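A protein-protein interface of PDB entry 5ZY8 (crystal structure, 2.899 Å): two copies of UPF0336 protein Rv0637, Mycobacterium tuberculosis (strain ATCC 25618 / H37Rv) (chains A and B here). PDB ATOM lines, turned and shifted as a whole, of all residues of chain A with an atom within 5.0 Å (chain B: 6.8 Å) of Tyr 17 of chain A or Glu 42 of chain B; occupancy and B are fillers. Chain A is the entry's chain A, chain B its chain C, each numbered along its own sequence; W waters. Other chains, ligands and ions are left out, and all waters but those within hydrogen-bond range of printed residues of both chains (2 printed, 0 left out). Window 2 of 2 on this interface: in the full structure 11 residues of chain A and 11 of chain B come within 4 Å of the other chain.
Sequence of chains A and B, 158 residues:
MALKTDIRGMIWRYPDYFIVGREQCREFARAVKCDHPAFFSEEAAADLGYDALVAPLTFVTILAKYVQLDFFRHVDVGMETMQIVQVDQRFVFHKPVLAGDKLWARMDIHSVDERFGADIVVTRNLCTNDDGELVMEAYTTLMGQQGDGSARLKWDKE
OD2 of Asp 16 of chain A is in salt-bridge range of NH2 of Arg 22 of chain B (2.8 Å). The side-chain carboxylate (OD2) of Asp 16 of chain A lies within salt-bridge range of the guanidinium group (NH2) of Arg 26 of chain B, at 2.9 Å. NH1 of Arg 22 of chain B is in hydrogen-bond range of O of Tyr 17 of chain A (2.8 Å). The side-chain carboxylate (OE1) of Glu 42 of chain B sits at hydrogen-bond distance from the side-chain hydroxyl (OH) of Tyr 17 of chain A. OE1 of Glu 23 of chain B is in hydrogen-bond range of N of Ile 19 of chain A.
The backbone carbonyl oxygen of Phe 18 of chain A lies within hydrogen-bond range of the backbone NH of Leu 103 of chain A (2.9 Å). The guanidinium group (NH1) of Arg 22 of chain B lies within salt-bridge range of the side-chain carboxylate (OE1) of Glu 23 of chain B (2.8 Å). The side-chain carboxylate (OE1) of Glu 42 of chain B is in salt-bridge range of the guanidinium group (NE) of Arg 22 of chain B, at 2.7 Å. OE2 of Glu 23 of chain B lies within salt-bridge range of NH2 of Arg 26 of chain B, at 2.9 Å. The guanidinium group (NH1) of Arg 26 of chain B sits at hydrogen-bond distance from the backbone carbonyl oxygen (O) of Phe 40 of chain B (2.9 Å).
Glu 23 of chain B touches Tyr 17 of chain A (OE1 to O, 3.8 Å). Phe 18 of chain A touches Glu 23 of chain B.
Glu 42 of chain B touches one residue of chain A. Of the printed residues of chain B, Phe 18 of chain A touches Glu 23. Printed residues of chain B within 4 Å of Asp 16 of chain A: Arg 22 and Arg 26. Pro 37 of chain B touches none of the printed residues of chain A. The nearest printed residue of chain A that does not touch Arg 26 of chain B is Tyr 17 of chain A (4.2 Å).
Hydrophobic or aromatic side chains of chain A that line the printed part of chain B: Tyr 17 and Phe 18. Of the 18 printed residues of chain B, 4 touch a printed residue of chain A. Printed residues of chain B that touch a printed residue of chain A: Arg 22, Glu 23, Arg 26 and Glu 42. Among the printed residues, 7 pairs touch across the chains. Among the printed residues, Asp or Glu carboxylates within 4 Å of a Lys or Arg side-chain nitrogen of the other chain: Asp 16 of chain A with Arg 22 of chain B and Asp 16 of chain A with Arg 26 of chain B.
No position is printed for both chains.
Water W2 lies within hydrogen-bond range of the backbone carbonyl oxygen of Tyr 17 of chain A (2.7 Å), the side-chain carboxylate of Glu 23 of chain B (3.3 Å) and the guanidinium group of Arg 26 of chain B (3.4 Å). Water W1 lies within hydrogen-bond range of the backbone carbonyl oxygen (O) of Ile 19 of chain A (2.9 Å), the backbone NH (N) of Glu 23 of chain B (3.0 Å) and the backbone NH (N) of Arg 22 of chain B (3.1 Å).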
ATOM      1  N   PRO A  15       1.984  -2.643   2.703  1.00  0.00           N
ATOM      2  CA  PRO A  15       1.013  -2.380   1.642  1.00  0.00           C
ATOM      3  C   PRO A  15      -0.050  -3.457   1.470  1.00  0.00           C
ATOM      4  O   PRO A  15      -0.874  -3.346   0.552  1.00  0.00           O
ATOM      5  CB  PRO A  15       1.907  -2.266   0.397  1.00  0.00           C
ATOM      6  CG  PRO A  15       3.064  -3.121   0.690  1.00  0.00           C
ATOM      7  CD  PRO A  15       3.306  -3.021   2.172  1.00  0.00           C
ATOM      8  N   ASP A  16      -0.063  -4.498   2.296  1.00  0.00           N
ATOM      9  CA  ASP A  16      -1.047  -5.556   2.153  1.00  0.00           C
ATOM     10  C   ASP A  16      -1.779  -5.783   3.467  1.00  0.00           C
ATOM     11  O   ASP A  16      -1.291  -5.436   4.543  1.00  0.00           O
ATOM     12  CB  ASP A  16      -0.394  -6.851   1.697  1.00  0.00           C
ATOM     13  CG  ASP A  16      -1.382  -7.793   1.056  1.00  0.00           C
ATOM     14  OD1 ASP A  16      -2.557  -7.389   0.872  1.00  0.00           O
ATOM     15  OD2 ASP A  16      -0.984  -8.937   0.739  1.00  0.00           O
ATOM     16  N   TYR A  17      -2.969  -6.372   3.365  1.00  0.00           N
ATOM     17  CA  TYR A  17      -3.681  -6.845   4.543  1.00  0.00           C
ATOM     18  C   TYR A  17      -3.268  -8.280   4.851  1.00  0.00           C
ATOM     19  O   TYR A  17      -2.619  -8.955   4.047  1.00  0.00           O
ATOM     20  CB  TYR A  17      -5.201  -6.739   4.366  1.00  0.00           C
ATOM     21  CG  TYR A  17      -5.809  -7.457   3.168  1.00  0.00           C
ATOM     22  CD1 TYR A  17      -6.103  -8.818   3.209  1.00  0.00           C
ATOM     23  CD2 TYR A  17      -6.142  -6.758   2.018  1.00  0.00           C
ATOM     24  CE1 TYR A  17      -6.682  -9.460   2.122  1.00  0.00           C
ATOM     25  CE2 TYR A  17      -6.716  -7.392   0.931  1.00  0.00           C
ATOM     26  CZ  TYR A  17      -6.985  -8.740   0.987  1.00  0.00           C
ATOM     27  OH  TYR A  17      -7.563  -9.365  -0.097  1.00  0.00           O
ATOM     28  N   PHE A  18      -3.639  -8.737   6.045  1.00  0.00           N
ATOM     29  CA  PHE A  18      -3.241 -10.045   6.552  1.00  0.00           C
ATOM     30  C   PHE A  18      -4.464 -10.766   7.117  1.00  0.00           C
ATOM     31  O   PHE A  18      -5.172 -10.218   7.969  1.00  0.00           O
ATOM     32  CB  PHE A  18      -2.141  -9.864   7.607  1.00  0.00           C
ATOM     33  CG  PHE A  18      -1.678 -11.139   8.254  1.00  0.00           C
ATOM     34  CD1 PHE A  18      -2.376 -11.696   9.330  1.00  0.00           C
ATOM     35  CD2 PHE A  18      -0.521 -11.764   7.815  1.00  0.00           C
ATOM     36  CE1 PHE A  18      -1.949 -12.866   9.925  1.00  0.00           C
ATOM     37  CE2 PHE A  18      -0.074 -12.932   8.423  1.00  0.00           C
ATOM     38  CZ  PHE A  18      -0.795 -13.483   9.480  1.00  0.00           C
ATOM     39  N   ILE A  19      -4.729 -11.976   6.629  1.00  0.00           N
ATOM     40  CA  ILE A  19      -5.847 -12.789   7.117  1.00  0.00           C
ATOM     41  C   ILE A  19      -5.342 -13.802   8.134  1.00  0.00           C
ATOM     42  O   ILE A  19      -4.386 -14.542   7.868  1.00  0.00           O
ATOM     43  CB  ILE A  19      -6.597 -13.488   5.966  1.00  0.00           C
ATOM     44  CG1 ILE A  19      -7.217 -12.447   5.033  1.00  0.00           C
ATOM     45  CG2 ILE A  19      -7.635 -14.443   6.525  1.00  0.00           C
ATOM     46  CD1 ILE A  19      -8.351 -11.693   5.670  1.00  0.00           C
ATOM     47  N   LYS A 102      -9.206  -9.746   9.633  1.00  0.00           N
ATOM     48  CA  LYS A 102      -8.448  -9.007   8.632  1.00  0.00           C
ATOM     49  C   LYS A 102      -7.689  -7.877   9.322  1.00  0.00           C
ATOM     50  O   LYS A 102      -8.307  -6.999   9.933  1.00  0.00           O
ATOM     51  CB  LYS A 102      -9.395  -8.452   7.569  1.00  0.00           C
ATOM     52  CG  LYS A 102      -8.722  -7.948   6.325  1.00  0.00           C
ATOM     53  CD  LYS A 102      -9.683  -7.076   5.557  1.00  0.00           C
ATOM     54  CE  LYS A 102      -9.263  -6.875   4.118  1.00  0.00           C
ATOM     55  NZ  LYS A 102     -10.303  -6.112   3.382  1.00  0.00           N
ATOM     56  N   LEU A 103      -6.359  -7.874   9.195  1.00  0.00           N
ATOM     57  CA  LEU A 103      -5.489  -6.957   9.932  1.00  0.00           C
ATOM     58  C   LEU A 103      -4.582  -6.142   9.014  1.00  0.00           C
ATOM     59  O   LEU A 103      -4.060  -6.648   8.014  1.00  0.00           O
ATOM     60  CB  LEU A 103      -4.613  -7.706  10.942  1.00  0.00           C
ATOM     61  CG  LEU A 103      -5.326  -8.482  12.046  1.00  0.00           C
ATOM     62  CD1 LEU A 103      -4.304  -8.998  13.038  1.00  0.00           C
ATOM     63  CD2 LEU A 103      -6.344  -7.593  12.743  1.00  0.00           C
ATOM     64  N   TRP A 104      -4.376  -4.883   9.391  1.00  0.00           N
ATOM     65  CA  TRP A 104      -3.468  -3.969   8.714  1.00  0.00           C
ATOM     66  C   TRP A 104      -2.293  -3.631   9.629  1.00  0.00           C
ATOM     67  O   TRP A 104      -2.477  -3.364  10.827  1.00  0.00           O
ATOM     68  CB  TRP A 104      -4.209  -2.703   8.299  1.00  0.00           C
ATOM     69  CG  TRP A 104      -5.348  -2.991   7.361  1.00  0.00           C
ATOM     70  CD1 TRP A 104      -6.656  -3.231   7.700  1.00  0.00           C
ATOM     71  CD2 TRP A 104      -5.277  -3.106   5.933  1.00  0.00           C
ATOM     72  NE1 TRP A 104      -7.402  -3.468   6.569  1.00  0.00           N
ATOM     73  CE2 TRP A 104      -6.584  -3.398   5.471  1.00  0.00           C
ATOM     74  CE3 TRP A 104      -4.241  -2.981   5.000  1.00  0.00           C
ATOM     75  CZ2 TRP A 104      -6.880  -3.570   4.113  1.00  0.00           C
ATOM     76  CZ3 TRP A 104      -4.536  -3.152   3.652  1.00  0.00           C
ATOM     77  CH2 TRP A 104      -5.849  -3.445   3.223  1.00  0.00           C
ATOM     78  N   ARG B  22      -5.559 -17.915   3.000  1.00  0.00           N
ATOM     79  CA  ARG B  22      -4.831 -17.027   2.089  1.00  0.00           C
ATOM     80  C   ARG B  22      -3.327 -17.040   2.354  1.00  0.00           C
ATOM     81  O   ARG B  22      -2.543 -17.464   1.495  1.00  0.00           O
ATOM     82  CB  ARG B  22      -5.382 -15.597   2.201  1.00  0.00           C
ATOM     83  CG  ARG B  22      -4.698 -14.557   1.306  1.00  0.00           C
ATOM     84  CD  ARG B  22      -5.303 -13.179   1.559  1.00  0.00           C
ATOM     85  NE  ARG B  22      -4.708 -12.102   0.762  1.00  0.00           N
ATOM     86  CZ  ARG B  22      -4.021 -11.076   1.266  1.00  0.00           C
ATOM     87  NH1 ARG B  22      -3.830 -10.985   2.572  1.00  0.00           N
ATOM     88  NH2 ARG B  22      -3.531 -10.136   0.472  1.00  0.00           N
ATOM     89  N   GLU B  23      -2.905 -16.598   3.550  1.00  0.00           N
ATOM     90  CA  GLU B  23      -1.470 -16.482   3.812  1.00  0.00           C
ATOM     91  C   GLU B  23      -0.790 -17.835   3.717  1.00  0.00           C
ATOM     92  O   GLU B  23       0.353 -17.936   3.245  1.00  0.00           O
ATOM     93  CB  GLU B  23      -1.187 -15.890   5.201  1.00  0.00           C
ATOM     94  CG  GLU B  23      -1.967 -14.644   5.643  1.00  0.00           C
ATOM     95  CD  GLU B  23      -1.887 -13.479   4.659  1.00  0.00           C
ATOM     96  OE1 GLU B  23      -2.881 -12.713   4.582  1.00  0.00           O
ATOM     97  OE2 GLU B  23      -0.831 -13.302   4.001  1.00  0.00           O
ATOM     98  N   ARG B  26      -0.091 -18.653   0.052  1.00  0.00           N
ATOM     99  CA  ARG B  26       1.052 -17.911  -0.464  1.00  0.00           C
ATOM    100  C   ARG B  26       2.374 -18.509   0.020  1.00  0.00           C
ATOM    101  O   ARG B  26       3.328 -18.622  -0.760  1.00  0.00           O
ATOM    102  CB  ARG B  26       0.914 -16.430  -0.117  1.00  0.00           C
ATOM    103  CG  ARG B  26      -0.182 -15.790  -0.970  1.00  0.00           C
ATOM    104  CD  ARG B  26      -0.146 -14.263  -1.042  1.00  0.00           C
ATOM    105  NE  ARG B  26      -0.259 -13.567   0.237  1.00  0.00           N
ATOM    106  CZ  ARG B  26      -0.663 -12.304   0.344  1.00  0.00           C
ATOM    107  NH1 ARG B  26      -0.992 -11.627  -0.750  1.00  0.00           N
ATOM    108  NH2 ARG B  26      -0.749 -11.722   1.534  1.00  0.00           N
ATOM    109  N   PRO B  37       1.698 -14.729 -10.726  1.00  0.00           N
ATOM    110  CA  PRO B  37       1.087 -13.729  -9.837  1.00  0.00           C
ATOM    111  C   PRO B  37      -0.335 -14.058  -9.375  1.00  0.00           C
ATOM    112  O   PRO B  37      -0.806 -13.426  -8.421  1.00  0.00           O
ATOM    113  CB  PRO B  37       1.111 -12.450 -10.685  1.00  0.00           C
ATOM    114  CG  PRO B  37       1.253 -12.919 -12.083  1.00  0.00           C
ATOM    115  CD  PRO B  37       2.100 -14.147 -12.011  1.00  0.00           C
ATOM    116  N   ALA B  38      -1.040 -14.998 -10.011  1.00  0.00           N
ATOM    117  CA  ALA B  38      -2.348 -15.380  -9.490  1.00  0.00           C
ATOM    118  C   ALA B  38      -2.236 -16.207  -8.209  1.00  0.00           C
ATOM    119  O   ALA B  38      -3.223 -16.348  -7.477  1.00  0.00           O
ATOM    120  CB  ALA B  38      -3.139 -16.149 -10.542  1.00  0.00           C
ATOM    121  N   PHE B  40      -0.411 -15.084  -5.772  1.00  0.00           N
ATOM    122  CA  PHE B  40      -0.060 -14.134  -4.718  1.00  0.00           C
ATOM    123  C   PHE B  40      -0.885 -12.844  -4.674  1.00  0.00           C
ATOM    124  O   PHE B  40      -0.944 -12.220  -3.604  1.00  0.00           O
ATOM    125  CB  PHE B  40       1.427 -13.770  -4.805  1.00  0.00           C
ATOM    126  CG  PHE B  40       2.334 -14.963  -4.817  1.00  0.00           C
ATOM    127  CD1 PHE B  40       2.752 -15.547  -3.630  1.00  0.00           C
ATOM    128  CD2 PHE B  40       2.778 -15.503  -6.020  1.00  0.00           C
ATOM    129  CE1 PHE B  40       3.601 -16.654  -3.635  1.00  0.00           C
ATOM    130  CE2 PHE B  40       3.625 -16.608  -6.041  1.00  0.00           C
ATOM    131  CZ  PHE B  40       4.039 -17.186  -4.843  1.00  0.00           C
ATOM    132  N   SER B  41      -1.494 -12.418  -5.780  1.00  0.00           N
ATOM    133  CA  SER B  41      -2.184 -11.135  -5.864  1.00  0.00           C
ATOM    134  C   SER B  41      -3.658 -11.322  -6.209  1.00  0.00           C
ATOM    135  O   SER B  41      -4.001 -12.134  -7.070  1.00  0.00           O
ATOM    136  CB  SER B  41      -1.528 -10.230  -6.905  1.00  0.00           C
ATOM    137  OG  SER B  41      -2.450  -9.266  -7.383  1.00  0.00           O
ATOM    138  N   GLU B  42      -4.531 -10.582  -5.511  1.00  0.00           N
ATOM    139  CA  GLU B  42      -5.954 -10.590  -5.850  1.00  0.00           C
ATOM    140  C   GLU B  42      -6.240  -9.850  -7.155  1.00  0.00           C
ATOM    141  O   GLU B  42      -7.203 -10.190  -7.853  1.00  0.00           O
ATOM    142  CB  GLU B  42      -6.770  -9.966  -4.718  1.00  0.00           C
ATOM    143  CG  GLU B  42      -7.030 -10.889  -3.555  1.00  0.00           C
ATOM    144  CD  GLU B  42      -5.903 -10.889  -2.546  1.00  0.00           C
ATOM    145  OE1 GLU B  42      -6.099 -11.462  -1.455  1.00  0.00           O
ATOM    146  OE2 GLU B  42      -4.821 -10.328  -2.838  1.00  0.00           O
ATOM    147  N   GLU B  43      -5.427  -8.846  -7.505  1.00  0.00           N
ATOM    148  CA  GLU B  43      -5.575  -8.195  -8.808  1.00  0.00           C
ATOM    149  C   GLU B  43      -5.253  -9.159  -9.947  1.00  0.00           C
ATOM    150  O   GLU B  43      -6.003  -9.251 -10.930  1.00  0.00           O
ATOM    151  CB  GLU B  43      -4.685  -6.949  -8.904  1.00  0.00           C
ATOM    152  CG  GLU B  43      -4.934  -5.845  -7.870  1.00  0.00           C
ATOM    153  CD  GLU B  43      -4.982  -4.448  -8.505  1.00  0.00           C
ATOM    154  OE1 GLU B  43      -4.554  -4.300  -9.677  1.00  0.00           O
ATOM    155  OE2 GLU B  43      -5.447  -3.498  -7.833  1.00  0.00           O
ATOM    156  N   ALA B  44      -4.129  -9.881  -9.832  1.00  0.00           N
ATOM    157  CA  ALA B  44      -3.739 -10.844 -10.859  1.00  0.00           C
ATOM    158  C   ALA B  44      -4.778 -11.945 -11.019  1.00  0.00           C
ATOM    159  O   ALA B  44      -5.107 -12.338 -12.144  1.00  0.00           O
ATOM    160  CB  ALA B  44      -2.377 -11.450 -10.521  1.00  0.00           C
ATOM    161  N   ALA B  45      -5.297 -12.463  -9.903  1.00  0.00           N
ATOM    162  CA  ALA B  45      -6.354 -13.467  -9.976  1.00  0.00           C
ATOM    163  C   ALA B  45      -7.636 -12.883 -10.559  1.00  0.00           C
ATOM    164  O   ALA B  45      -8.353 -13.564 -11.308  1.00  0.00           O
ATOM    165  CB  ALA B  45      -6.612 -14.061  -8.592  1.00  0.00           C
ATOM    166  N   ALA B  46      -7.950 -11.629 -10.224  1.00  0.00           N
ATOM    167  CA  ALA B  46      -9.117 -10.987 -10.819  1.00  0.00           C
ATOM    168  C   ALA B  46      -8.959 -10.847 -12.330  1.00  0.00           C
ATOM    169  O   ALA B  46      -9.927 -11.018 -13.086  1.00  0.00           O
ATOM    170  CB  ALA B  46      -9.357  -9.626 -10.168  1.00  0.00           C
ATOM    171  N   ASP B  47      -7.737 -10.556 -12.787  1.00  0.00           N
ATOM    172  CA  ASP B  47      -7.492 -10.443 -14.220  1.00  0.00           C
ATOM    173  C   ASP B  47      -7.821 -11.738 -14.947  1.00  0.00           C
ATOM    174  O   ASP B  47      -8.188 -11.710 -16.126  1.00  0.00           O
ATOM    175  CB  ASP B  47      -6.037 -10.043 -14.484  1.00  0.00           C
ATOM    176  CG  ASP B  47      -5.762  -8.586 -14.155  1.00  0.00           C
ATOM    177  OD1 ASP B  47      -6.676  -7.757 -14.364  1.00  0.00           O
ATOM    178  OD2 ASP B  47      -4.634  -8.271 -13.708  1.00  0.00           O
ATOM    179  N   TYR B  50     -10.990 -14.679 -11.249  1.00  0.00           N
ATOM    180  CA  TYR B  50     -11.235 -15.242  -9.927  1.00  0.00           C
ATOM    181  C   TYR B  50     -11.323 -14.140  -8.879  1.00  0.00           C
ATOM    182  O   TYR B  50     -10.557 -13.173  -8.916  1.00  0.00           O
ATOM    183  CB  TYR B  50     -10.135 -16.239  -9.577  1.00  0.00           C
ATOM    184  CG  TYR B  50      -9.772 -17.163 -10.733  1.00  0.00           C
ATOM    185  CD1 TYR B  50      -8.449 -17.504 -10.985  1.00  0.00           C
ATOM    186  CD2 TYR B  50     -10.753 -17.726 -11.546  1.00  0.00           C
ATOM    187  CE1 TYR B  50      -8.115 -18.357 -12.029  1.00  0.00           C
ATOM    188  CE2 TYR B  50     -10.427 -18.579 -12.593  1.00  0.00           C
ATOM    189  CZ  TYR B  50      -9.110 -18.892 -12.829  1.00  0.00           C
ATOM    190  OH  TYR B  50      -8.802 -19.732 -13.877  1.00  0.00           O
ATOM    191  N   ASP B  51     -12.261 -14.292  -7.941  1.00  0.00           N
ATOM    192  CA  ASP B  51     -12.516 -13.287  -6.914  1.00  0.00           C
ATOM    193  C   ASP B  51     -11.756 -13.552  -5.610  1.00  0.00           C
ATOM    194  O   ASP B  51     -11.954 -12.820  -4.632  1.00  0.00           O
ATOM    195  CB  ASP B  51     -14.021 -13.164  -6.656  1.00  0.00           C
ATOM    196  CG  ASP B  51     -14.685 -14.496  -6.383  1.00  0.00           C
ATOM    197  OD1 ASP B  51     -13.987 -15.535  -6.408  1.00  0.00           O
ATOM    198  OD2 ASP B  51     -15.914 -14.496  -6.146  1.00  0.00           O
ATOM    199  N   ALA B  52     -10.900 -14.577  -5.585  1.00  0.00           N
ATOM    200  CA  ALA B  52      -9.879 -14.779  -4.562  1.00  0.00           C
ATOM    201  C   ALA B  52      -8.650 -15.350  -5.258  1.00  0.00           C
ATOM    202  O   ALA B  52      -8.661 -15.592  -6.465  1.00  0.00           O
ATOM    203  CB  ALA B  52     -10.369 -15.692  -3.435  1.00  0.00           C
ATOM    204  N   LEU B  53      -7.566 -15.543  -4.516  1.00  0.00           N
ATOM    205  CA  LEU B  53      -6.360 -16.102  -5.116  1.00  0.00           C
ATOM    206  C   LEU B  53      -6.524 -17.591  -5.372  1.00  0.00           C
ATOM    207  O   LEU B  53      -7.318 -18.275  -4.719  1.00  0.00           O
ATOM    208  CB  LEU B  53      -5.135 -15.936  -4.210  1.00  0.00           C
ATOM    209  CG  LEU B  53      -4.620 -14.607  -3.664  1.00  0.00           C
ATOM    210  CD1 LEU B  53      -5.598 -14.074  -2.666  1.00  0.00           C
ATOM    211  CD2 LEU B  53      -3.250 -14.778  -3.015  1.00  0.00           C
ATOM    212  N   ALA B  99      -8.471 -19.289  -2.289  1.00  0.00           N
ATOM    213  CA  ALA B  99      -8.349 -18.867  -0.907  1.00  0.00           C
ATOM    214  C   ALA B  99      -9.720 -18.443  -0.399  1.00  0.00           C
ATOM    215  O   ALA B  99     -10.497 -17.797  -1.114  1.00  0.00           O
ATOM    216  CB  ALA B  99      -7.348 -17.722  -0.788  1.00  0.00           C
HETATM  217  O   HOH W   1      -4.967 -16.505   5.749  1.00  0.00           O
HETATM  218  O   HOH W   2      -0.287 -10.125   4.521  1.00  0.00           O
